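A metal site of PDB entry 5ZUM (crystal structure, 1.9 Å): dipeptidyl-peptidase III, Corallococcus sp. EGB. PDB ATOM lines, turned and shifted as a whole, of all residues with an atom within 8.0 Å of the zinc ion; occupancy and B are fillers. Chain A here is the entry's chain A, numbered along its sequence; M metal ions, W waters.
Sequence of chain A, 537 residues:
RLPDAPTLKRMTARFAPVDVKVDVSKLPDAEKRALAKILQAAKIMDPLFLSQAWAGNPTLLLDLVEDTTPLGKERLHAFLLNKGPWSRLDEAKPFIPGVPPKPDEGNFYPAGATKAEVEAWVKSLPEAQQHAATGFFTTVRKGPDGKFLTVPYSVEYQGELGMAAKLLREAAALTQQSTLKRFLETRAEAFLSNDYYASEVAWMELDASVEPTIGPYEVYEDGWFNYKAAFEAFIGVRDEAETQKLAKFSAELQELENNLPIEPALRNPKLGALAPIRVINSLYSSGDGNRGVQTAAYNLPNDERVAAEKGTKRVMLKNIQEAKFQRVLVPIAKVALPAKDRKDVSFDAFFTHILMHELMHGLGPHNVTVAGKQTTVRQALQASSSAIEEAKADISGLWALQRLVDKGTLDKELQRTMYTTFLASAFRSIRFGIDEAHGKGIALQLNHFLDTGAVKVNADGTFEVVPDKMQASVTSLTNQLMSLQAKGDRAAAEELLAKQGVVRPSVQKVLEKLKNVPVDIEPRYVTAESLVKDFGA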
ATOM      1  N   GLU A 218      -8.610 -11.307 -22.385  1.00  0.00           N
ATOM      2  CA  GLU A 218      -8.157 -10.036 -21.827  1.00  0.00           C
ATOM      3  C   GLU A 218      -9.246  -9.258 -21.095  1.00  0.00           C
ATOM      4  O   GLU A 218     -10.459  -9.394 -21.355  1.00  0.00           O
ATOM      5  CB  GLU A 218      -7.494  -9.142 -22.892  1.00  0.00           C
ATOM      6  CG  GLU A 218      -6.431  -9.790 -23.783  1.00  0.00           C
ATOM      7  CD  GLU A 218      -5.160 -10.191 -23.043  1.00  0.00           C
ATOM      8  OE1 GLU A 218      -5.022  -9.769 -21.869  1.00  0.00           O
ATOM      9  OE2 GLU A 218      -4.244 -10.747 -23.715  1.00  0.00           O
ATOM     10  N   TYR A 220      -9.240  -5.816 -20.497  1.00  0.00           N
ATOM     11  CA  TYR A 220      -9.227  -4.377 -20.752  1.00  0.00           C
ATOM     12  C   TYR A 220     -10.636  -3.781 -20.890  1.00  0.00           C
ATOM     13  O   TYR A 220     -10.850  -2.599 -20.606  1.00  0.00           O
ATOM     14  CB  TYR A 220      -8.406  -4.003 -21.989  1.00  0.00           C
ATOM     15  CG  TYR A 220      -7.008  -4.607 -22.107  1.00  0.00           C
ATOM     16  CD1 TYR A 220      -5.945  -4.137 -21.329  1.00  0.00           C
ATOM     17  CD2 TYR A 220      -6.719  -5.485 -23.136  1.00  0.00           C
ATOM     18  CE1 TYR A 220      -4.670  -4.650 -21.485  1.00  0.00           C
ATOM     19  CE2 TYR A 220      -5.447  -6.016 -23.315  1.00  0.00           C
ATOM     20  CZ  TYR A 220      -4.425  -5.620 -22.477  1.00  0.00           C
ATOM     21  OH  TYR A 220      -3.155  -6.110 -22.705  1.00  0.00           O
ATOM     22  N   ALA A 297       1.390  -8.971 -30.369  1.00  0.00           N
ATOM     23  CA  ALA A 297       1.856 -10.198 -29.723  1.00  0.00           C
ATOM     24  C   ALA A 297       1.129 -10.332 -28.411  1.00  0.00           C
ATOM     25  O   ALA A 297       0.548  -9.372 -27.885  1.00  0.00           O
ATOM     26  CB  ALA A 297       3.346 -10.061 -29.474  1.00  0.00           C
ATOM     27  N   TYR A 298       1.277 -11.487 -27.787  1.00  0.00           N
ATOM     28  CA  TYR A 298       0.566 -11.701 -26.548  1.00  0.00           C
ATOM     29  C   TYR A 298       1.171 -12.820 -25.677  1.00  0.00           C
ATOM     30  O   TYR A 298       1.999 -13.614 -26.170  1.00  0.00           O
ATOM     31  CB  TYR A 298      -0.922 -11.938 -26.837  1.00  0.00           C
ATOM     32  CG  TYR A 298      -1.238 -13.002 -27.798  1.00  0.00           C
ATOM     33  CD1 TYR A 298      -1.454 -14.313 -27.378  1.00  0.00           C
ATOM     34  CD2 TYR A 298      -1.371 -12.719 -29.140  1.00  0.00           C
ATOM     35  CE1 TYR A 298      -1.805 -15.301 -28.299  1.00  0.00           C
ATOM     36  CE2 TYR A 298      -1.668 -13.690 -30.049  1.00  0.00           C
ATOM     37  CZ  TYR A 298      -1.908 -14.983 -29.619  1.00  0.00           C
ATOM     38  OH  TYR A 298      -2.218 -15.968 -30.531  1.00  0.00           O
ATOM     39  N   ASN A 299       0.740 -12.848 -24.433  1.00  0.00           N
ATOM     40  CA  ASN A 299       1.175 -13.809 -23.418  1.00  0.00           C
ATOM     41  C   ASN A 299      -0.076 -14.337 -22.711  1.00  0.00           C
ATOM     42  O   ASN A 299      -0.787 -13.588 -22.072  1.00  0.00           O
ATOM     43  CB  ASN A 299       2.104 -13.126 -22.412  1.00  0.00           C
ATOM     44  CG  ASN A 299       2.527 -14.049 -21.290  1.00  0.00           C
ATOM     45  OD1 ASN A 299       3.221 -15.032 -21.524  1.00  0.00           O
ATOM     46  ND2 ASN A 299       2.045 -13.792 -20.079  1.00  0.00           N
ATOM     47  N   ILE A 354       9.533  -6.422 -28.257  1.00  0.00           N
ATOM     48  CA  ILE A 354       8.193  -6.946 -28.135  1.00  0.00           C
ATOM     49  C   ILE A 354       8.280  -8.351 -27.493  1.00  0.00           C
ATOM     50  O   ILE A 354       7.557  -8.626 -26.622  1.00  0.00           O
ATOM     51  CB  ILE A 354       7.422  -6.916 -29.463  1.00  0.00           C
ATOM     52  CG1 ILE A 354       7.148  -5.475 -29.905  1.00  0.00           C
ATOM     53  CG2 ILE A 354       6.127  -7.654 -29.349  1.00  0.00           C
ATOM     54  CD1 ILE A 354       6.575  -5.378 -31.281  1.00  0.00           C
ATOM     55  N   HIS A 357       8.908  -7.967 -23.879  1.00  0.00           N
ATOM     56  CA  HIS A 357       7.659  -7.513 -23.299  1.00  0.00           C
ATOM     57  C   HIS A 357       6.774  -8.693 -22.985  1.00  0.00           C
ATOM     58  O   HIS A 357       6.285  -8.817 -21.866  1.00  0.00           O
ATOM     59  CB  HIS A 357       6.981  -6.569 -24.303  1.00  0.00           C
ATOM     60  CG  HIS A 357       5.641  -6.064 -23.879  1.00  0.00           C
ATOM     61  ND1 HIS A 357       5.392  -4.718 -23.690  1.00  0.00           N
ATOM     62  CD2 HIS A 357       4.445  -6.675 -23.817  1.00  0.00           C
ATOM     63  CE1 HIS A 357       4.114  -4.560 -23.355  1.00  0.00           C
ATOM     64  NE2 HIS A 357       3.514  -5.726 -23.470  1.00  0.00           N
ATOM     65  N   GLU A 358       6.614  -9.580 -23.954  1.00  0.00           N
ATOM     66  CA  GLU A 358       5.794 -10.782 -23.735  1.00  0.00           C
ATOM     67  C   GLU A 358       6.402 -11.741 -22.747  1.00  0.00           C
ATOM     68  O   GLU A 358       5.661 -12.346 -21.968  1.00  0.00           O
ATOM     69  CB  GLU A 358       5.450 -11.503 -25.048  1.00  0.00           C
ATOM     70  CG  GLU A 358       4.626 -10.716 -26.048  1.00  0.00           C
ATOM     71  CD  GLU A 358       3.398 -10.015 -25.496  1.00  0.00           C
ATOM     72  OE1 GLU A 358       2.894 -10.396 -24.436  1.00  0.00           O
ATOM     73  OE2 GLU A 358       2.956  -9.031 -26.134  1.00  0.00           O
ATOM     74  N   MET A 360       8.252 -10.837 -20.150  1.00  0.00           N
ATOM     75  CA  MET A 360       8.165 -10.233 -18.844  1.00  0.00           C
ATOM     76  C   MET A 360       6.743 -10.054 -18.351  1.00  0.00           C
ATOM     77  O   MET A 360       6.560 -10.010 -17.136  1.00  0.00           O
ATOM     78  CB  MET A 360       8.822  -8.860 -18.837  1.00  0.00           C
ATOM     79  CG  MET A 360      10.289  -8.870 -19.188  1.00  0.00           C
ATOM     80  SD  MET A 360      11.273 -10.148 -18.045  1.00  0.00           S
ATOM     81  CE  MET A 360      11.303  -9.094 -16.394  1.00  0.00           C
ATOM     82  N   HIS A 361       5.741 -10.162 -19.216  1.00  0.00           N
ATOM     83  CA  HIS A 361       4.360 -10.245 -18.683  1.00  0.00           C
ATOM     84  C   HIS A 361       4.291 -11.435 -17.740  1.00  0.00           C
ATOM     85  O   HIS A 361       3.514 -11.451 -16.789  1.00  0.00           O
ATOM     86  CB  HIS A 361       3.315 -10.458 -19.801  1.00  0.00           C
ATOM     87  CG  HIS A 361       2.651  -9.197 -20.258  1.00  0.00           C
ATOM     88  ND1 HIS A 361       2.138  -8.274 -19.378  1.00  0.00           N
ATOM     89  CD2 HIS A 361       2.399  -8.710 -21.501  1.00  0.00           C
ATOM     90  CE1 HIS A 361       1.632  -7.263 -20.058  1.00  0.00           C
ATOM     91  NE2 HIS A 361       1.712  -7.536 -21.351  1.00  0.00           N
ATOM     92  N   SER A 386      -4.259  -2.597 -15.716  1.00  0.00           N
ATOM     93  CA  SER A 386      -3.865  -2.831 -17.089  1.00  0.00           C
ATOM     94  C   SER A 386      -2.712  -1.953 -17.533  1.00  0.00           C
ATOM     95  O   SER A 386      -1.710  -2.413 -18.080  1.00  0.00           O
ATOM     96  CB  SER A 386      -5.098  -2.612 -18.004  1.00  0.00           C
ATOM     97  OG  SER A 386      -5.959  -3.740 -17.935  1.00  0.00           O
ATOM     98  N   GLU A 389       0.449  -2.948 -15.621  1.00  0.00           N
ATOM     99  CA  GLU A 389       1.026  -4.188 -16.161  1.00  0.00           C
ATOM    100  C   GLU A 389       1.657  -3.956 -17.519  1.00  0.00           C
ATOM    101  O   GLU A 389       2.725  -4.538 -17.804  1.00  0.00           O
ATOM    102  CB  GLU A 389       0.000  -5.329 -16.166  1.00  0.00           C
ATOM    103  CG  GLU A 389       0.478  -6.673 -16.755  1.00  0.00           C
ATOM    104  CD  GLU A 389       1.709  -7.294 -16.077  1.00  0.00           C
ATOM    105  OE1 GLU A 389       2.085  -6.968 -14.935  1.00  0.00           O
ATOM    106  OE2 GLU A 389       2.334  -8.205 -16.693  1.00  0.00           O
ATOM    107  N   GLU A 390       1.041  -3.123 -18.406  1.00  0.00           N
ATOM    108  CA  GLU A 390       1.689  -2.847 -19.678  1.00  0.00           C
ATOM    109  C   GLU A 390       3.009  -2.055 -19.538  1.00  0.00           C
ATOM    110  O   GLU A 390       3.982  -2.357 -20.236  1.00  0.00           O
ATOM    111  CB  GLU A 390       0.800  -2.144 -20.703  1.00  0.00           C
ATOM    112  CG  GLU A 390      -0.421  -2.974 -21.106  1.00  0.00           C
ATOM    113  CD  GLU A 390      -0.012  -4.315 -21.674  1.00  0.00           C
ATOM    114  OE1 GLU A 390       1.023  -4.379 -22.347  1.00  0.00           O
ATOM    115  OE2 GLU A 390      -0.779  -5.263 -21.518  1.00  0.00           O
ATOM    116  N   ALA A 391       3.046  -1.082 -18.635  1.00  0.00           N
ATOM    117  CA  ALA A 391       4.275  -0.334 -18.380  1.00  0.00           C
ATOM    118  C   ALA A 391       5.340  -1.270 -17.819  1.00  0.00           C
ATOM    119  O   ALA A 391       6.468  -1.260 -18.295  1.00  0.00           O
ATOM    120  CB  ALA A 391       4.024   0.776 -17.382  1.00  0.00           C
ATOM    121  N   LYS A 392       4.948  -2.118 -16.873  1.00  0.00           N
ATOM    122  CA  LYS A 392       5.864  -3.128 -16.356  1.00  0.00           C
ATOM    123  C   LYS A 392       6.492  -3.996 -17.433  1.00  0.00           C
ATOM    124  O   LYS A 392       7.716  -4.278 -17.400  1.00  0.00           O
ATOM    125  CB  LYS A 392       5.154  -4.045 -15.360  1.00  0.00           C
ATOM    126  CG  LYS A 392       6.129  -4.935 -14.599  1.00  0.00           C
ATOM    127  CD  LYS A 392       5.604  -6.321 -14.367  1.00  0.00           C
ATOM    128  CE  LYS A 392       5.547  -7.162 -15.623  1.00  0.00           C
ATOM    129  NZ  LYS A 392       4.856  -8.466 -15.286  1.00  0.00           N
ATOM    130  N   ALA A 393       5.646  -4.543 -18.297  1.00  0.00           N
ATOM    131  CA  ALA A 393       6.144  -5.422 -19.360  1.00  0.00           C
ATOM    132  C   ALA A 393       7.079  -4.687 -20.322  1.00  0.00           C
ATOM    133  O   ALA A 393       8.140  -5.205 -20.729  1.00  0.00           O
ATOM    134  CB  ALA A 393       4.996  -6.077 -20.130  1.00  0.00           C
ATOM    135  N   ASP A 394       6.718  -3.460 -20.685  1.00  0.00           N
ATOM    136  CA  ASP A 394       7.604  -2.676 -21.554  1.00  0.00           C
ATOM    137  C   ASP A 394       8.945  -2.375 -20.874  1.00  0.00           C
ATOM    138  O   ASP A 394      10.003  -2.635 -21.443  1.00  0.00           O
ATOM    139  CB  ASP A 394       6.940  -1.338 -21.935  1.00  0.00           C
ATOM    140  CG  ASP A 394       6.031  -1.438 -23.118  1.00  0.00           C
ATOM    141  OD1 ASP A 394       6.265  -2.269 -24.027  1.00  0.00           O
ATOM    142  OD2 ASP A 394       5.147  -0.551 -23.192  1.00  0.00           O
ATOM    143  N   ALA A 437      -4.505   1.219 -22.433  1.00  0.00           N
ATOM    144  CA  ALA A 437      -3.485   0.693 -21.544  1.00  0.00           C
ATOM    145  C   ALA A 437      -2.047   0.859 -22.009  1.00  0.00           C
ATOM    146  O   ALA A 437      -1.236   1.339 -21.300  1.00  0.00           O
ATOM    147  CB  ALA A 437      -3.785  -0.732 -21.134  1.00  0.00           C
ATOM    148  N   HIS A 438      -1.776   0.480 -23.228  1.00  0.00           N
ATOM    149  CA  HIS A 438      -0.422   0.610 -23.743  1.00  0.00           C
ATOM    150  C   HIS A 438       0.038   2.088 -23.781  1.00  0.00           C
ATOM    151  O   HIS A 438       1.119   2.385 -23.420  1.00  0.00           O
ATOM    152  CB  HIS A 438      -0.281  -0.046 -25.083  1.00  0.00           C
ATOM    153  CG  HIS A 438      -0.667  -1.484 -25.091  1.00  0.00           C
ATOM    154  ND1 HIS A 438      -1.931  -1.915 -25.405  1.00  0.00           N
ATOM    155  CD2 HIS A 438       0.057  -2.578 -24.809  1.00  0.00           C
ATOM    156  CE1 HIS A 438      -1.960  -3.227 -25.329  1.00  0.00           C
ATOM    157  NE2 HIS A 438      -0.760  -3.650 -24.968  1.00  0.00           N
HETATM  158 ZN    ZN M   1       1.486  -6.300 -22.973  1.00  0.00          ZN
HETATM  159  O   HOH W   1       0.295  -6.994 -24.762  1.00  0.00           O
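The side-chain carboxylate of Glu 390 sits close to a ring nitrogen (NE2) of His 438, 3.3 Å away.
ND1 of His 361 sits at hydrogen-bond distance from OE2 of Glu 389 (2.7 Å).
A ring nitrogen (ND1) of His 357 is in hydrogen-bond range of the side-chain carboxylate of Asp 394.
The side-chain carboxylate (OE2) of Glu 390 lies within hydrogen-bond range of the side-chain hydroxyl (OH) of Tyr 220.
Of the 19 residues printed, 3 come within 4 Å of the zinc ion.
The nearest printed residue that does not touch the zinc ion is His 438 (4.01 Å).
The zinc ion is bound by NE2 of His 361 (2.1 Å), OE1 of Glu 390 (2.1 Å), NE2 of His 357 (2.2 Å) and water W1 (2.3 Å).
The zinc ion has four donor atoms within binding distance.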
